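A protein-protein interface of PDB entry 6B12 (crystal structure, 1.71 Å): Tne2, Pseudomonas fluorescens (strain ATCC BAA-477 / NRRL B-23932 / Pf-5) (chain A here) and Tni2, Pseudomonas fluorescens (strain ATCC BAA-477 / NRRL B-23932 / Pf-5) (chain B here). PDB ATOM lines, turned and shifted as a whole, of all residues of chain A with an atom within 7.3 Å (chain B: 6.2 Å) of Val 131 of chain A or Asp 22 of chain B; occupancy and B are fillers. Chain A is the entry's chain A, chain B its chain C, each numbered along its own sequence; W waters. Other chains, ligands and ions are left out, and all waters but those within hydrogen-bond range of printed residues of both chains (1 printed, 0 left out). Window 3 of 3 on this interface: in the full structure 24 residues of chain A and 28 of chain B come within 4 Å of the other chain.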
ATOM      1  N   MET A  48     -14.102   4.052  16.822  1.00  0.00           N
ATOM      2  CA  MET A  48     -12.767   3.614  16.425  1.00  0.00           C
ATOM      3  C   MET A  48     -12.777   2.225  15.791  1.00  0.00           C
ATOM      4  O   MET A  48     -11.840   1.876  15.064  1.00  0.00           O
ATOM      5  CB  MET A  48     -11.815   3.633  17.623  1.00  0.00           C
ATOM      6  CG  MET A  48     -11.271   5.010  17.968  1.00  0.00           C
ATOM      7  SD  MET A  48     -10.516   5.975  16.444  1.00  0.00           S
ATOM      8  CE  MET A  48      -8.987   4.826  16.038  1.00  0.00           C
ATOM      9  N   ILE A  63     -16.652  22.732  20.508  1.00  0.00           N
ATOM     10  CA  ILE A  63     -16.883  22.306  21.887  1.00  0.00           C
ATOM     11  C   ILE A  63     -15.535  22.332  22.598  1.00  0.00           C
ATOM     12  O   ILE A  63     -14.721  21.423  22.409  1.00  0.00           O
ATOM     13  CB  ILE A  63     -17.527  20.914  21.942  1.00  0.00           C
ATOM     14  CG1 ILE A  63     -18.831  20.903  21.132  1.00  0.00           C
ATOM     15  CG2 ILE A  63     -17.844  20.537  23.370  1.00  0.00           C
ATOM     16  CD1 ILE A  63     -19.436  19.511  21.026  1.00  0.00           C
ATOM     17  N   PRO A  64     -15.250  23.355  23.389  1.00  0.00           N
ATOM     18  CA  PRO A  64     -13.875  23.564  23.861  1.00  0.00           C
ATOM     19  C   PRO A  64     -13.422  22.656  24.997  1.00  0.00           C
ATOM     20  O   PRO A  64     -12.216  22.421  25.149  1.00  0.00           O
ATOM     21  CB  PRO A  64     -13.887  25.028  24.322  1.00  0.00           C
ATOM     22  CG  PRO A  64     -15.125  25.651  23.681  1.00  0.00           C
ATOM     23  CD  PRO A  64     -16.111  24.525  23.626  1.00  0.00           C
ATOM     24  N   SER A  65     -14.332  22.167  25.828  1.00  0.00           N
ATOM     25  CA  SER A  65     -13.880  21.463  27.026  1.00  0.00           C
ATOM     26  C   SER A  65     -14.972  20.533  27.522  1.00  0.00           C
ATOM     27  O   SER A  65     -16.133  20.648  27.135  1.00  0.00           O
ATOM     28  CB  SER A  65     -13.517  22.442  28.136  1.00  0.00           C
ATOM     29  OG  SER A  65     -14.698  22.996  28.692  1.00  0.00           O
ATOM     30  N   GLN A  66     -14.586  19.622  28.423  1.00  0.00           N
ATOM     31  CA  GLN A  66     -15.587  18.795  29.089  1.00  0.00           C
ATOM     32  C   GLN A  66     -16.495  19.629  29.981  1.00  0.00           C
ATOM     33  O   GLN A  66     -17.693  19.340  30.087  1.00  0.00           O
ATOM     34  CB  GLN A  66     -14.906  17.691  29.902  1.00  0.00           C
ATOM     35  CG  GLN A  66     -14.004  16.795  29.075  1.00  0.00           C
ATOM     36  CD  GLN A  66     -13.316  15.729  29.913  1.00  0.00           C
ATOM     37  OE1 GLN A  66     -13.876  15.238  30.892  1.00  0.00           O
ATOM     38  NE2 GLN A  66     -12.091  15.370  29.532  1.00  0.00           N
ATOM     39  N   VAL A  83     -17.014  12.196  29.038  1.00  0.00           N
ATOM     40  CA  VAL A  83     -17.200  13.080  27.889  1.00  0.00           C
ATOM     41  C   VAL A  83     -15.837  13.547  27.406  1.00  0.00           C
ATOM     42  O   VAL A  83     -15.670  14.713  27.044  1.00  0.00           O
ATOM     43  CB  VAL A  83     -18.108  14.280  28.221  1.00  0.00           C
ATOM     44  CG1 VAL A  83     -19.556  13.826  28.407  1.00  0.00           C
ATOM     45  CG2 VAL A  83     -17.612  15.050  29.467  1.00  0.00           C
ATOM     46  N   SER A  84     -14.848  12.651  27.405  1.00  0.00           N
ATOM     47  CA  SER A  84     -13.487  13.081  27.123  1.00  0.00           C
ATOM     48  C   SER A  84     -13.151  13.100  25.638  1.00  0.00           C
ATOM     49  O   SER A  84     -12.021  13.436  25.281  1.00  0.00           O
ATOM     50  CB  SER A  84     -12.481  12.198  27.873  1.00  0.00           C
ATOM     51  OG  SER A  84     -12.385  10.921  27.284  1.00  0.00           O
ATOM     52  N   HIS A  85     -14.088  12.771  24.755  1.00  0.00           N
ATOM     53  CA  HIS A  85     -13.807  12.808  23.329  1.00  0.00           C
ATOM     54  C   HIS A  85     -14.918  13.540  22.588  1.00  0.00           C
ATOM     55  O   HIS A  85     -16.071  13.575  23.027  1.00  0.00           O
ATOM     56  CB  HIS A  85     -13.648  11.392  22.741  1.00  0.00           C
ATOM     57  CG  HIS A  85     -12.417  10.677  23.212  1.00  0.00           C
ATOM     58  ND1 HIS A  85     -12.396   9.901  24.350  1.00  0.00           N
ATOM     59  CD2 HIS A  85     -11.161  10.638  22.706  1.00  0.00           C
ATOM     60  CE1 HIS A  85     -11.183   9.408  24.522  1.00  0.00           C
ATOM     61  NE2 HIS A  85     -10.414   9.836  23.537  1.00  0.00           N
ATOM     62  N   VAL A  86     -14.547  14.117  21.456  1.00  0.00           N
ATOM     63  CA  VAL A  86     -15.470  14.812  20.568  1.00  0.00           C
ATOM     64  C   VAL A  86     -15.178  14.347  19.152  1.00  0.00           C
ATOM     65  O   VAL A  86     -14.022  14.083  18.803  1.00  0.00           O
ATOM     66  CB  VAL A  86     -15.330  16.347  20.696  1.00  0.00           C
ATOM     67  CG1 VAL A  86     -13.940  16.811  20.261  1.00  0.00           C
ATOM     68  CG2 VAL A  86     -16.414  17.076  19.876  1.00  0.00           C
ATOM     69  N   THR A 128     -10.729  11.344  13.066  1.00  0.00           N
ATOM     70  CA  THR A 128     -10.778  10.492  14.242  1.00  0.00           C
ATOM     71  C   THR A 128     -11.286  11.298  15.427  1.00  0.00           C
ATOM     72  O   THR A 128     -11.288  12.533  15.389  1.00  0.00           O
ATOM     73  CB  THR A 128      -9.393   9.914  14.562  1.00  0.00           C
ATOM     74  OG1 THR A 128      -8.532  10.969  15.006  1.00  0.00           O
ATOM     75  CG2 THR A 128      -8.790   9.257  13.327  1.00  0.00           C
ATOM     76  N   PRO A 129     -11.745  10.639  16.489  1.00  0.00           N
ATOM     77  CA  PRO A 129     -12.123  11.383  17.693  1.00  0.00           C
ATOM     78  C   PRO A 129     -10.991  12.282  18.166  1.00  0.00           C
ATOM     79  O   PRO A 129      -9.806  11.966  18.013  1.00  0.00           O
ATOM     80  CB  PRO A 129     -12.424  10.280  18.711  1.00  0.00           C
ATOM     81  CG  PRO A 129     -12.851   9.119  17.875  1.00  0.00           C
ATOM     82  CD  PRO A 129     -12.076   9.207  16.600  1.00  0.00           C
ATOM     83  N   GLY A 130     -11.372  13.419  18.728  1.00  0.00           N
ATOM     84  CA  GLY A 130     -10.423  14.312  19.354  1.00  0.00           C
ATOM     85  C   GLY A 130     -10.585  14.275  20.855  1.00  0.00           C
ATOM     86  O   GLY A 130     -11.622  13.840  21.359  1.00  0.00           O
ATOM     87  N   VAL A 131      -9.579  14.721  21.586  1.00  0.00           N
ATOM     88  CA  VAL A 131      -9.636  14.715  23.038  1.00  0.00           C
ATOM     89  C   VAL A 131     -10.214  16.042  23.509  1.00  0.00           C
ATOM     90  O   VAL A 131      -9.818  17.110  23.026  1.00  0.00           O
ATOM     91  CB  VAL A 131      -8.245  14.467  23.642  1.00  0.00           C
ATOM     92  CG1 VAL A 131      -8.299  14.597  25.152  1.00  0.00           C
ATOM     93  CG2 VAL A 131      -7.752  13.089  23.240  1.00  0.00           C
ATOM     94  N   LEU A 132     -11.173  15.977  24.434  1.00  0.00           N
ATOM     95  CA  LEU A 132     -11.675  17.182  25.082  1.00  0.00           C
ATOM     96  C   LEU A 132     -10.877  17.438  26.349  1.00  0.00           C
ATOM     97  O   LEU A 132     -10.835  16.562  27.224  1.00  0.00           O
ATOM     98  CB  LEU A 132     -13.145  17.046  25.437  1.00  0.00           C
ATOM     99  CG  LEU A 132     -14.205  17.285  24.381  1.00  0.00           C
ATOM    100  CD1 LEU A 132     -15.572  17.324  25.053  1.00  0.00           C
ATOM    101  CD2 LEU A 132     -13.922  18.595  23.652  1.00  0.00           C
ATOM    102  N   PRO A 133     -10.247  18.598  26.499  1.00  0.00           N
ATOM    103  CA  PRO A 133      -9.622  18.925  27.785  1.00  0.00           C
ATOM    104  C   PRO A 133     -10.691  19.006  28.863  1.00  0.00           C
ATOM    105  O   PRO A 133     -11.830  19.404  28.602  1.00  0.00           O
ATOM    106  CB  PRO A 133      -8.982  20.296  27.537  1.00  0.00           C
ATOM    107  CG  PRO A 133      -9.074  20.539  26.052  1.00  0.00           C
ATOM    108  CD  PRO A 133     -10.209  19.723  25.554  1.00  0.00           C
ATOM    109  N   VAL A 134     -10.311  18.638  30.087  1.00  0.00           N
ATOM    110  CA  VAL A 134     -11.268  18.701  31.191  1.00  0.00           C
ATOM    111  C   VAL A 134     -11.778  20.125  31.368  1.00  0.00           C
ATOM    112  O   VAL A 134     -12.979  20.353  31.573  1.00  0.00           O
ATOM    113  CB  VAL A 134     -10.634  18.161  32.487  1.00  0.00           C
ATOM    114  CG1 VAL A 134     -11.630  18.242  33.623  1.00  0.00           C
ATOM    115  CG2 VAL A 134     -10.172  16.719  32.288  1.00  0.00           C
ATOM    116  N   THR B  20      -6.910   1.735  24.891  1.00  0.00           N
ATOM    117  CA  THR B  20      -7.826   2.869  24.847  1.00  0.00           C
ATOM    118  C   THR B  20      -7.880   3.501  23.457  1.00  0.00           C
ATOM    119  O   THR B  20      -6.997   3.310  22.618  1.00  0.00           O
ATOM    120  CB  THR B  20      -7.424   3.929  25.864  1.00  0.00           C
ATOM    121  OG1 THR B  20      -6.169   4.494  25.477  1.00  0.00           O
ATOM    122  CG2 THR B  20      -7.307   3.323  27.260  1.00  0.00           C
ATOM    123  N   VAL B  21      -8.948   4.276  23.229  1.00  0.00           N
ATOM    124  CA  VAL B  21      -9.052   5.067  22.006  1.00  0.00           C
ATOM    125  C   VAL B  21      -7.831   5.959  21.829  1.00  0.00           C
ATOM    126  O   VAL B  21      -7.298   6.086  20.724  1.00  0.00           O
ATOM    127  CB  VAL B  21     -10.361   5.882  22.022  1.00  0.00           C
ATOM    128  CG1 VAL B  21     -10.341   6.990  20.966  1.00  0.00           C
ATOM    129  CG2 VAL B  21     -11.529   4.926  21.823  1.00  0.00           C
ATOM    130  N   ASP B  22      -7.354   6.575  22.916  1.00  0.00           N
ATOM    131  CA  ASP B  22      -6.214   7.484  22.791  1.00  0.00           C
ATOM    132  C   ASP B  22      -4.948   6.737  22.393  1.00  0.00           C
ATOM    133  O   ASP B  22      -4.112   7.267  21.652  1.00  0.00           O
ATOM    134  CB  ASP B  22      -5.995   8.247  24.092  1.00  0.00           C
ATOM    135  CG  ASP B  22      -7.116   9.235  24.379  1.00  0.00           C
ATOM    136  OD1 ASP B  22      -7.738   9.719  23.408  1.00  0.00           O
ATOM    137  OD2 ASP B  22      -7.378   9.511  25.569  1.00  0.00           O
ATOM    138  N   GLN B  23      -4.785   5.509  22.886  1.00  0.00           N
ATOM    139  CA  GLN B  23      -3.635   4.708  22.483  1.00  0.00           C
ATOM    140  C   GLN B  23      -3.698   4.373  20.998  1.00  0.00           C
ATOM    141  O   GLN B  23      -2.677   4.409  20.300  1.00  0.00           O
ATOM    142  CB  GLN B  23      -3.566   3.446  23.352  1.00  0.00           C
ATOM    143  CG  GLN B  23      -3.125   3.775  24.782  1.00  0.00           C
ATOM    144  CD  GLN B  23      -3.301   2.634  25.774  1.00  0.00           C
ATOM    145  OE1 GLN B  23      -4.059   1.696  25.544  1.00  0.00           O
ATOM    146  NE2 GLN B  23      -2.596   2.727  26.899  1.00  0.00           N
ATOM    147  N   MET B  24      -4.886   4.071  20.487  1.00  0.00           N
ATOM    148  CA  MET B  24      -5.036   3.781  19.073  1.00  0.00           C
ATOM    149  C   MET B  24      -4.683   4.989  18.221  1.00  0.00           C
ATOM    150  O   MET B  24      -3.990   4.865  17.212  1.00  0.00           O
ATOM    151  CB  MET B  24      -6.468   3.335  18.765  1.00  0.00           C
ATOM    152  CG  MET B  24      -6.880   2.084  19.503  1.00  0.00           C
ATOM    153  SD  MET B  24      -8.791   1.743  19.153  1.00  0.00           S
ATOM    154  CE  MET B  24      -8.654   0.717  17.515  1.00  0.00           C
ATOM    155  N   ILE B  25      -5.180   6.160  18.626  1.00  0.00           N
ATOM    156  CA  ILE B  25      -4.886   7.378  17.880  1.00  0.00           C
ATOM    157  C   ILE B  25      -3.391   7.670  17.911  1.00  0.00           C
ATOM    158  O   ILE B  25      -2.792   8.018  16.885  1.00  0.00           O
ATOM    159  CB  ILE B  25      -5.716   8.550  18.435  1.00  0.00           C
ATOM    160  CG1 ILE B  25      -7.205   8.324  18.139  1.00  0.00           C
ATOM    161  CG2 ILE B  25      -5.220   9.883  17.881  1.00  0.00           C
ATOM    162  CD1 ILE B  25      -8.116   9.089  19.044  1.00  0.00           C
ATOM    163  N   ALA B  26      -2.762   7.507  19.080  1.00  0.00           N
ATOM    164  CA  ALA B  26      -1.331   7.772  19.215  1.00  0.00           C
ATOM    165  C   ALA B  26      -0.487   6.871  18.328  1.00  0.00           C
ATOM    166  O   ALA B  26       0.654   7.222  18.009  1.00  0.00           O
ATOM    167  CB  ALA B  26      -0.896   7.606  20.673  1.00  0.00           C
ATOM    168  N   LEU B  27      -1.005   5.713  17.943  1.00  0.00           N
ATOM    169  CA  LEU B  27      -0.312   4.845  17.006  1.00  0.00           C
ATOM    170  C   LEU B  27      -0.563   5.237  15.562  1.00  0.00           C
ATOM    171  O   LEU B  27      -0.011   4.600  14.659  1.00  0.00           O
ATOM    172  CB  LEU B  27      -0.725   3.392  17.234  1.00  0.00           C
ATOM    173  CG  LEU B  27      -0.286   2.871  18.603  1.00  0.00           C
ATOM    174  CD1 LEU B  27      -0.690   1.434  18.789  1.00  0.00           C
ATOM    175  CD2 LEU B  27       1.221   3.034  18.750  1.00  0.00           C
HETATM  176  O   HOH W   1      -9.056  11.089  26.636  1.00  0.00           O
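A ring nitrogen (NE2) of His 85 of chain A lies within hydrogen-bond range of the side-chain carboxylate (OD1) of Asp 22 of chain B (2.7 Å).
Among the printed residues, merely in contact across the chains: Val 131 of chain A with Asp 22 of chain B (3.4 Å), Pro 129 of chain A with Ile 25 of chain B (3.5 Å), Met 48 of chain A with Val 21 of chain B (3.7 Å), His 85 of chain A with Val 21 of chain B (3.8 Å) and Met 48 of chain A with Met 24 of chain B (3.9 Å).
Water W1 lies within hydrogen-bond range of the side-chain carboxylate (OD2) of Asp 22 of chain B and the side-chain hydroxyl (OG) of Ser 84 of chain A.
Val 131 of chain A touches just one residue of chain B: Asp 22.
Of chain A, only His 85 (2.7 Å) and Val 131 (3.4 Å) come within 4 Å of Asp 22 of chain B.
Printed residues of chain A within 4 Å of Met 24 of chain B: Met 48.
Of the printed residues of chain A, Ile 25 of chain B touches Pro 129.
Of the printed residues of chain B, His 85 of chain A touches Val 21 (3.8 Å) and Asp 22 (2.7 Å).
Of the printed residues of chain B, Pro 129 of chain A touches Ile 25 (3.5 Å).
The nearest residue of chain B that does not touch Val 131 of chain A is Ile 25 of chain B (5.8 Å).
The nearest residue of chain A that does not touch Asp 22 of chain B is Ser 84 of chain A (5.5 Å).
The nearest printed residue of chain B that does not touch Met 48 of chain A is Ile 25 of chain B (4.4 Å).
Of the 16 printed residues of chain A, 4 touch a printed residue of chain B.
Hydrophobic or aromatic side chains of chain A within 4 Å of the printed part of chain B: Met 48, His 85 and Val 131.
Hydrophobic or aromatic side chains of chain B that line the printed part of chain A: Val 21, Met 24 and Ile 25.
The side-chain hydroxyl (OG) of Ser 84 of chain A is in hydrogen-bond range of a ring nitrogen (ND1) of His 85 of chain A (3.1 Å).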
